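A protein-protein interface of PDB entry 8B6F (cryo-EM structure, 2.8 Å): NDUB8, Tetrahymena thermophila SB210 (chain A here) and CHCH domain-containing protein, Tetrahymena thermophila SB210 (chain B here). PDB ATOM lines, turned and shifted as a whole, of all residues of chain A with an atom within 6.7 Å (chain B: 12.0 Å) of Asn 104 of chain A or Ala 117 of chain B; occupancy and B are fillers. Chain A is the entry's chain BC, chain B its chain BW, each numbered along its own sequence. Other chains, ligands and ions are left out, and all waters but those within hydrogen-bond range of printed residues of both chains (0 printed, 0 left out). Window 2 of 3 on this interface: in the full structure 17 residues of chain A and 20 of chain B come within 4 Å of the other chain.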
ATOM      1  N   GLY A  99     -21.964  16.077   0.294  1.00  0.00           N
ATOM      2  CA  GLY A  99     -20.640  16.586  -0.009  1.00  0.00           C
ATOM      3  C   GLY A  99     -19.806  15.585  -0.781  1.00  0.00           C
ATOM      4  O   GLY A  99     -19.119  15.944  -1.740  1.00  0.00           O
ATOM      5  N   PHE A 100     -19.854  14.315  -0.378  1.00  0.00           N
ATOM      6  CA  PHE A 100     -19.103  13.290  -1.092  1.00  0.00           C
ATOM      7  C   PHE A 100     -19.556  13.189  -2.542  1.00  0.00           C
ATOM      8  O   PHE A 100     -18.728  13.069  -3.452  1.00  0.00           O
ATOM      9  CB  PHE A 100     -19.262  11.946  -0.384  1.00  0.00           C
ATOM     10  CG  PHE A 100     -18.375  10.868  -0.925  1.00  0.00           C
ATOM     11  CD1 PHE A 100     -18.757  10.130  -2.032  1.00  0.00           C
ATOM     12  CD2 PHE A 100     -17.161  10.585  -0.322  1.00  0.00           C
ATOM     13  CE1 PHE A 100     -17.944   9.134  -2.534  1.00  0.00           C
ATOM     14  CE2 PHE A 100     -16.342   9.591  -0.818  1.00  0.00           C
ATOM     15  CZ  PHE A 100     -16.733   8.864  -1.926  1.00  0.00           C
ATOM     16  N   TYR A 101     -20.867  13.231  -2.778  1.00  0.00           N
ATOM     17  CA  TYR A 101     -21.373  13.160  -4.144  1.00  0.00           C
ATOM     18  C   TYR A 101     -21.117  14.453  -4.905  1.00  0.00           C
ATOM     19  O   TYR A 101     -21.013  14.437  -6.136  1.00  0.00           O
ATOM     20  CB  TYR A 101     -22.865  12.836  -4.135  1.00  0.00           C
ATOM     21  CG  TYR A 101     -23.158  11.353  -4.108  1.00  0.00           C
ATOM     22  CD1 TYR A 101     -23.243  10.620  -5.284  1.00  0.00           C
ATOM     23  CD2 TYR A 101     -23.350  10.688  -2.905  1.00  0.00           C
ATOM     24  CE1 TYR A 101     -23.512   9.265  -5.261  1.00  0.00           C
ATOM     25  CE2 TYR A 101     -23.620   9.335  -2.872  1.00  0.00           C
ATOM     26  CZ  TYR A 101     -23.700   8.630  -4.053  1.00  0.00           C
ATOM     27  OH  TYR A 101     -23.969   7.283  -4.025  1.00  0.00           O
ATOM     28  N   PHE A 102     -21.017  15.578  -4.195  1.00  0.00           N
ATOM     29  CA  PHE A 102     -20.830  16.863  -4.859  1.00  0.00           C
ATOM     30  C   PHE A 102     -19.394  17.053  -5.332  1.00  0.00           C
ATOM     31  O   PHE A 102     -19.163  17.632  -6.398  1.00  0.00           O
ATOM     32  CB  PHE A 102     -21.235  17.993  -3.912  1.00  0.00           C
ATOM     33  CG  PHE A 102     -21.008  19.367  -4.472  1.00  0.00           C
ATOM     34  CD1 PHE A 102     -21.944  19.955  -5.307  1.00  0.00           C
ATOM     35  CD2 PHE A 102     -19.865  20.078  -4.145  1.00  0.00           C
ATOM     36  CE1 PHE A 102     -21.737  21.224  -5.817  1.00  0.00           C
ATOM     37  CE2 PHE A 102     -19.652  21.346  -4.650  1.00  0.00           C
ATOM     38  CZ  PHE A 102     -20.589  21.921  -5.487  1.00  0.00           C
ATOM     39  N   ILE A 103     -18.419  16.578  -4.560  1.00  0.00           N
ATOM     40  CA  ILE A 103     -17.015  16.752  -4.912  1.00  0.00           C
ATOM     41  C   ILE A 103     -16.546  15.582  -5.767  1.00  0.00           C
ATOM     42  O   ILE A 103     -15.349  15.444  -6.036  1.00  0.00           O
ATOM     43  CB  ILE A 103     -16.137  16.896  -3.653  1.00  0.00           C
ATOM     44  CG1 ILE A 103     -16.110  15.578  -2.864  1.00  0.00           C
ATOM     45  CG2 ILE A 103     -16.644  18.053  -2.798  1.00  0.00           C
ATOM     46  CD1 ILE A 103     -15.374  15.645  -1.534  1.00  0.00           C
ATOM     47  N   ASN A 104     -17.480  14.726  -6.197  1.00  0.00           N
ATOM     48  CA  ASN A 104     -17.112  13.547  -6.971  1.00  0.00           C
ATOM     49  C   ASN A 104     -18.058  13.262  -8.131  1.00  0.00           C
ATOM     50  O   ASN A 104     -18.011  12.157  -8.684  1.00  0.00           O
ATOM     51  CB  ASN A 104     -17.050  12.315  -6.062  1.00  0.00           C
ATOM     52  CG  ASN A 104     -16.010  12.448  -4.968  1.00  0.00           C
ATOM     53  OD1 ASN A 104     -14.941  13.016  -5.177  1.00  0.00           O
ATOM     54  ND2 ASN A 104     -16.321  11.919  -3.790  1.00  0.00           N
ATOM     55  N   THR A 105     -18.913  14.205  -8.517  1.00  0.00           N
ATOM     56  CA  THR A 105     -19.841  13.996  -9.620  1.00  0.00           C
ATOM     57  C   THR A 105     -20.096  15.328 -10.310  1.00  0.00           C
ATOM     58  O   THR A 105     -19.778  16.395  -9.783  1.00  0.00           O
ATOM     59  CB  THR A 105     -21.170  13.384  -9.154  1.00  0.00           C
ATOM     60  OG1 THR A 105     -21.815  14.275  -8.234  1.00  0.00           O
ATOM     61  CG2 THR A 105     -20.955  12.031  -8.488  1.00  0.00           C
ATOM     62  N   THR A 106     -20.677  15.250 -11.502  1.00  0.00           N
ATOM     63  CA  THR A 106     -21.038  16.419 -12.285  1.00  0.00           C
ATOM     64  C   THR A 106     -22.481  16.298 -12.753  1.00  0.00           C
ATOM     65  O   THR A 106     -22.992  15.185 -12.909  1.00  0.00           O
ATOM     66  CB  THR A 106     -20.111  16.582 -13.502  1.00  0.00           C
ATOM     67  OG1 THR A 106     -20.606  17.620 -14.358  1.00  0.00           O
ATOM     68  CG2 THR A 106     -20.016  15.288 -14.288  1.00  0.00           C
ATOM     69  N   TRP B  93     -14.533  13.770 -21.029  1.00  0.00           N
ATOM     70  CA  TRP B  93     -14.042  12.908 -19.959  1.00  0.00           C
ATOM     71  C   TRP B  93     -12.693  12.304 -20.323  1.00  0.00           C
ATOM     72  O   TRP B  93     -11.777  12.265 -19.495  1.00  0.00           O
ATOM     73  CB  TRP B  93     -15.064  11.809 -19.667  1.00  0.00           C
ATOM     74  CG  TRP B  93     -14.770  11.011 -18.432  1.00  0.00           C
ATOM     75  CD1 TRP B  93     -13.923   9.948 -18.323  1.00  0.00           C
ATOM     76  CD2 TRP B  93     -15.331  11.213 -17.127  1.00  0.00           C
ATOM     77  NE1 TRP B  93     -13.919   9.477 -17.032  1.00  0.00           N
ATOM     78  CE2 TRP B  93     -14.776  10.236 -16.279  1.00  0.00           C
ATOM     79  CE3 TRP B  93     -16.247  12.127 -16.597  1.00  0.00           C
ATOM     80  CZ2 TRP B  93     -15.104  10.148 -14.929  1.00  0.00           C
ATOM     81  CZ3 TRP B  93     -16.575  12.036 -15.255  1.00  0.00           C
ATOM     82  CH2 TRP B  93     -16.004  11.053 -14.436  1.00  0.00           C
ATOM     83  N   TYR B 108     -20.658  23.226 -23.323  1.00  0.00           N
ATOM     84  CA  TYR B 108     -20.457  22.200 -22.305  1.00  0.00           C
ATOM     85  C   TYR B 108     -19.093  22.311 -21.638  1.00  0.00           C
ATOM     86  O   TYR B 108     -18.962  22.000 -20.449  1.00  0.00           O
ATOM     87  CB  TYR B 108     -20.622  20.810 -22.920  1.00  0.00           C
ATOM     88  CG  TYR B 108     -20.522  19.693 -21.908  1.00  0.00           C
ATOM     89  CD1 TYR B 108     -21.612  19.346 -21.122  1.00  0.00           C
ATOM     90  CD2 TYR B 108     -19.339  18.991 -21.737  1.00  0.00           C
ATOM     91  CE1 TYR B 108     -21.526  18.329 -20.195  1.00  0.00           C
ATOM     92  CE2 TYR B 108     -19.244  17.972 -20.812  1.00  0.00           C
ATOM     93  CZ  TYR B 108     -20.340  17.646 -20.044  1.00  0.00           C
ATOM     94  OH  TYR B 108     -20.252  16.632 -19.122  1.00  0.00           O
ATOM     95  N   SER B 111     -18.646  24.609 -18.402  1.00  0.00           N
ATOM     96  CA  SER B 111     -19.252  24.165 -17.156  1.00  0.00           C
ATOM     97  C   SER B 111     -18.821  22.767 -16.735  1.00  0.00           C
ATOM     98  O   SER B 111     -19.073  22.383 -15.588  1.00  0.00           O
ATOM     99  CB  SER B 111     -20.784  24.204 -17.269  1.00  0.00           C
ATOM    100  OG  SER B 111     -21.240  23.369 -18.319  1.00  0.00           O
ATOM    101  N   PHE B 112     -18.184  22.001 -17.617  1.00  0.00           N
ATOM    102  CA  PHE B 112     -17.758  20.655 -17.260  1.00  0.00           C
ATOM    103  C   PHE B 112     -16.702  20.701 -16.164  1.00  0.00           C
ATOM    104  O   PHE B 112     -15.791  21.534 -16.186  1.00  0.00           O
ATOM    105  CB  PHE B 112     -17.210  19.929 -18.489  1.00  0.00           C
ATOM    106  CG  PHE B 112     -16.619  18.585 -18.180  1.00  0.00           C
ATOM    107  CD1 PHE B 112     -17.436  17.489 -17.961  1.00  0.00           C
ATOM    108  CD2 PHE B 112     -15.247  18.415 -18.114  1.00  0.00           C
ATOM    109  CE1 PHE B 112     -16.895  16.249 -17.677  1.00  0.00           C
ATOM    110  CE2 PHE B 112     -14.702  17.178 -17.830  1.00  0.00           C
ATOM    111  CZ  PHE B 112     -15.526  16.094 -17.612  1.00  0.00           C
ATOM    112  N   ARG B 113     -16.827  19.789 -15.200  1.00  0.00           N
ATOM    113  CA  ARG B 113     -15.855  19.672 -14.113  1.00  0.00           C
ATOM    114  C   ARG B 113     -15.902  18.228 -13.621  1.00  0.00           C
ATOM    115  O   ARG B 113     -16.820  17.851 -12.888  1.00  0.00           O
ATOM    116  CB  ARG B 113     -16.159  20.655 -12.992  1.00  0.00           C
ATOM    117  CG  ARG B 113     -15.109  20.670 -11.893  1.00  0.00           C
ATOM    118  CD  ARG B 113     -15.565  21.493 -10.700  1.00  0.00           C
ATOM    119  NE  ARG B 113     -16.716  20.896 -10.034  1.00  0.00           N
ATOM    120  CZ  ARG B 113     -17.302  21.395  -8.954  1.00  0.00           C
ATOM    121  NH1 ARG B 113     -16.869  22.508  -8.384  1.00  0.00           N
ATOM    122  NH2 ARG B 113     -18.347  20.761  -8.431  1.00  0.00           N
ATOM    123  N   LYS B 114     -14.915  17.434 -14.024  1.00  0.00           N
ATOM    124  CA  LYS B 114     -14.873  16.039 -13.615  1.00  0.00           C
ATOM    125  C   LYS B 114     -14.638  15.929 -12.114  1.00  0.00           C
ATOM    126  O   LYS B 114     -13.947  16.751 -11.507  1.00  0.00           O
ATOM    127  CB  LYS B 114     -13.779  15.291 -14.377  1.00  0.00           C
ATOM    128  CG  LYS B 114     -13.640  13.831 -13.977  1.00  0.00           C
ATOM    129  CD  LYS B 114     -13.039  12.993 -15.096  1.00  0.00           C
ATOM    130  CE  LYS B 114     -11.638  13.455 -15.460  1.00  0.00           C
ATOM    131  NZ  LYS B 114     -11.044  12.607 -16.532  1.00  0.00           N
ATOM    132  N   GLY B 115     -15.225  14.896 -11.515  1.00  0.00           N
ATOM    133  CA  GLY B 115     -15.105  14.722 -10.081  1.00  0.00           C
ATOM    134  C   GLY B 115     -13.662  14.551  -9.650  1.00  0.00           C
ATOM    135  O   GLY B 115     -12.842  13.959 -10.353  1.00  0.00           O
ATOM    136  N   LEU B 116     -13.353  15.089  -8.468  1.00  0.00           N
ATOM    137  CA  LEU B 116     -11.994  14.993  -7.948  1.00  0.00           C
ATOM    138  C   LEU B 116     -11.586  13.547  -7.711  1.00  0.00           C
ATOM    139  O   LEU B 116     -10.400  13.213  -7.810  1.00  0.00           O
ATOM    140  CB  LEU B 116     -11.874  15.798  -6.653  1.00  0.00           C
ATOM    141  CG  LEU B 116     -10.539  15.702  -5.908  1.00  0.00           C
ATOM    142  CD1 LEU B 116      -9.382  16.121  -6.797  1.00  0.00           C
ATOM    143  CD2 LEU B 116     -10.576  16.547  -4.648  1.00  0.00           C
ATOM    144  N   ALA B 117     -12.546  12.676  -7.398  1.00  0.00           N
ATOM    145  CA  ALA B 117     -12.220  11.276  -7.165  1.00  0.00           C
ATOM    146  C   ALA B 117     -11.734  10.595  -8.435  1.00  0.00           C
ATOM    147  O   ALA B 117     -10.897   9.688  -8.368  1.00  0.00           O
ATOM    148  CB  ALA B 117     -13.434  10.538  -6.603  1.00  0.00           C
ATOM    149  N   TRP B 118     -12.245  11.007  -9.590  1.00  0.00           N
ATOM    150  CA  TRP B 118     -11.875  10.391 -10.863  1.00  0.00           C
ATOM    151  C   TRP B 118     -10.692  11.106 -11.508  1.00  0.00           C
ATOM    152  O   TRP B 118     -10.738  11.501 -12.670  1.00  0.00           O
ATOM    153  CB  TRP B 118     -13.079  10.379 -11.796  1.00  0.00           C
ATOM    154  CG  TRP B 118     -14.367  10.088 -11.095  1.00  0.00           C
ATOM    155  CD1 TRP B 118     -15.392  10.959 -10.867  1.00  0.00           C
ATOM    156  CD2 TRP B 118     -14.760   8.842 -10.513  1.00  0.00           C
ATOM    157  NE1 TRP B 118     -16.403  10.327 -10.183  1.00  0.00           N
ATOM    158  CE2 TRP B 118     -16.039   9.028  -9.953  1.00  0.00           C
ATOM    159  CE3 TRP B 118     -14.155   7.587 -10.412  1.00  0.00           C
ATOM    160  CZ2 TRP B 118     -16.724   8.004  -9.305  1.00  0.00           C
ATOM    161  CZ3 TRP B 118     -14.833   6.576  -9.770  1.00  0.00           C
ATOM    162  CH2 TRP B 118     -16.106   6.786  -9.224  1.00  0.00           C
ATOM    163  N   LEU B 119      -9.610  11.269 -10.748  1.00  0.00           N
ATOM    164  CA  LEU B 119      -8.415  11.953 -11.237  1.00  0.00           C
ATOM    165  C   LEU B 119      -7.419  10.924 -11.769  1.00  0.00           C
ATOM    166  O   LEU B 119      -6.340  10.704 -11.218  1.00  0.00           O
ATOM    167  CB  LEU B 119      -7.799  12.800 -10.129  1.00  0.00           C
ATOM    168  CG  LEU B 119      -6.608  13.676 -10.524  1.00  0.00           C
ATOM    169  CD1 LEU B 119      -7.029  14.753 -11.513  1.00  0.00           C
ATOM    170  CD2 LEU B 119      -5.967  14.298  -9.295  1.00  0.00           C
ATOM    171  N   ASN B 120      -7.807  10.292 -12.869  1.00  0.00           N
ATOM    172  CA  ASN B 120      -6.965   9.290 -13.503  1.00  0.00           C
ATOM    173  C   ASN B 120      -5.684   9.922 -14.034  1.00  0.00           C
ATOM    174  O   ASN B 120      -5.593  11.139 -14.179  1.00  0.00           O
ATOM    175  CB  ASN B 120      -7.721   8.600 -14.637  1.00  0.00           C
ATOM    176  CG  ASN B 120      -6.899   7.529 -15.314  1.00  0.00           C
ATOM    177  OD1 ASN B 120      -6.351   7.740 -16.395  1.00  0.00           O
ATOM    178  ND2 ASN B 120      -6.798   6.370 -14.675  1.00  0.00           N
ATOM    179  OXT ASN B 120      -4.709   9.232 -14.327  1.00  0.00           O
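Hydrophobic or aromatic side chains of chain B within 4 Å of the printed part of chain A: Leu 116, Ala 117 and Trp 118.
Hydrophobic or aromatic side chains of chain A that line the printed part of chain B: Phe 102.
Among the printed residues, 6 pairs touch across the chains.
Among the printed residues, pairs that only touch across the chains: Phe 102 of chain A with Arg 113 of chain B (3.8 Å), Asn 104 of chain A with Gly 115 of chain B (3.8 Å) and Thr 106 of chain A with Arg 113 of chain B (3.6 Å).
N of Ala 117 of chain B sits close to OD1 of Asn 104 of chain A (3.3 Å).
O of Ile 103 of chain A sits at hydrogen-bond distance from N of Leu 116 of chain B.
The backbone carbonyl oxygen of Asn 104 of chain A lies within hydrogen-bond range of the indole nitrogen of Trp 118 of chain B, 2.9 Å away.
The side-chain amide nitrogen (ND2) of Asn 104 of chain A sits at hydrogen-bond distance from the backbone carbonyl oxygen (O) of Phe 100 of chain A (2.7 Å).
No residue of chain B comes within 4 Å of Phe 100 of chain A.
Phe 102 of chain A touches just one residue of chain B: Arg 113 (3.8 Å).
Of the printed residues of chain B, Ile 103 of chain A touches Leu 116.
Of chain B, only Gly 115, Ala 117 and Trp 118 come within 4 Å of Asn 104 of chain A.
No residue of chain B comes within 4 Å of Thr 105 of chain A.
Of the printed residues of chain A, Gly 115 of chain B touches Asn 104.
Of the printed residues of chain A, Leu 116 of chain B touches Ile 103 (3.2 Å).
Ala 117 of chain B touches just one residue of chain A: Asn 104.
Of the printed residues of chain A, Trp 118 of chain B touches Asn 104.
Asn 120 of chain B touches none of the printed residues of chain A.
The nearest residue of chain A that does not touch Ala 117 of chain B is Ile 103 of chain A (4.2 Å).
The nearest printed residue of chain A that does not touch Arg 113 of chain B is Thr 105 of chain A (4.5 Å).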
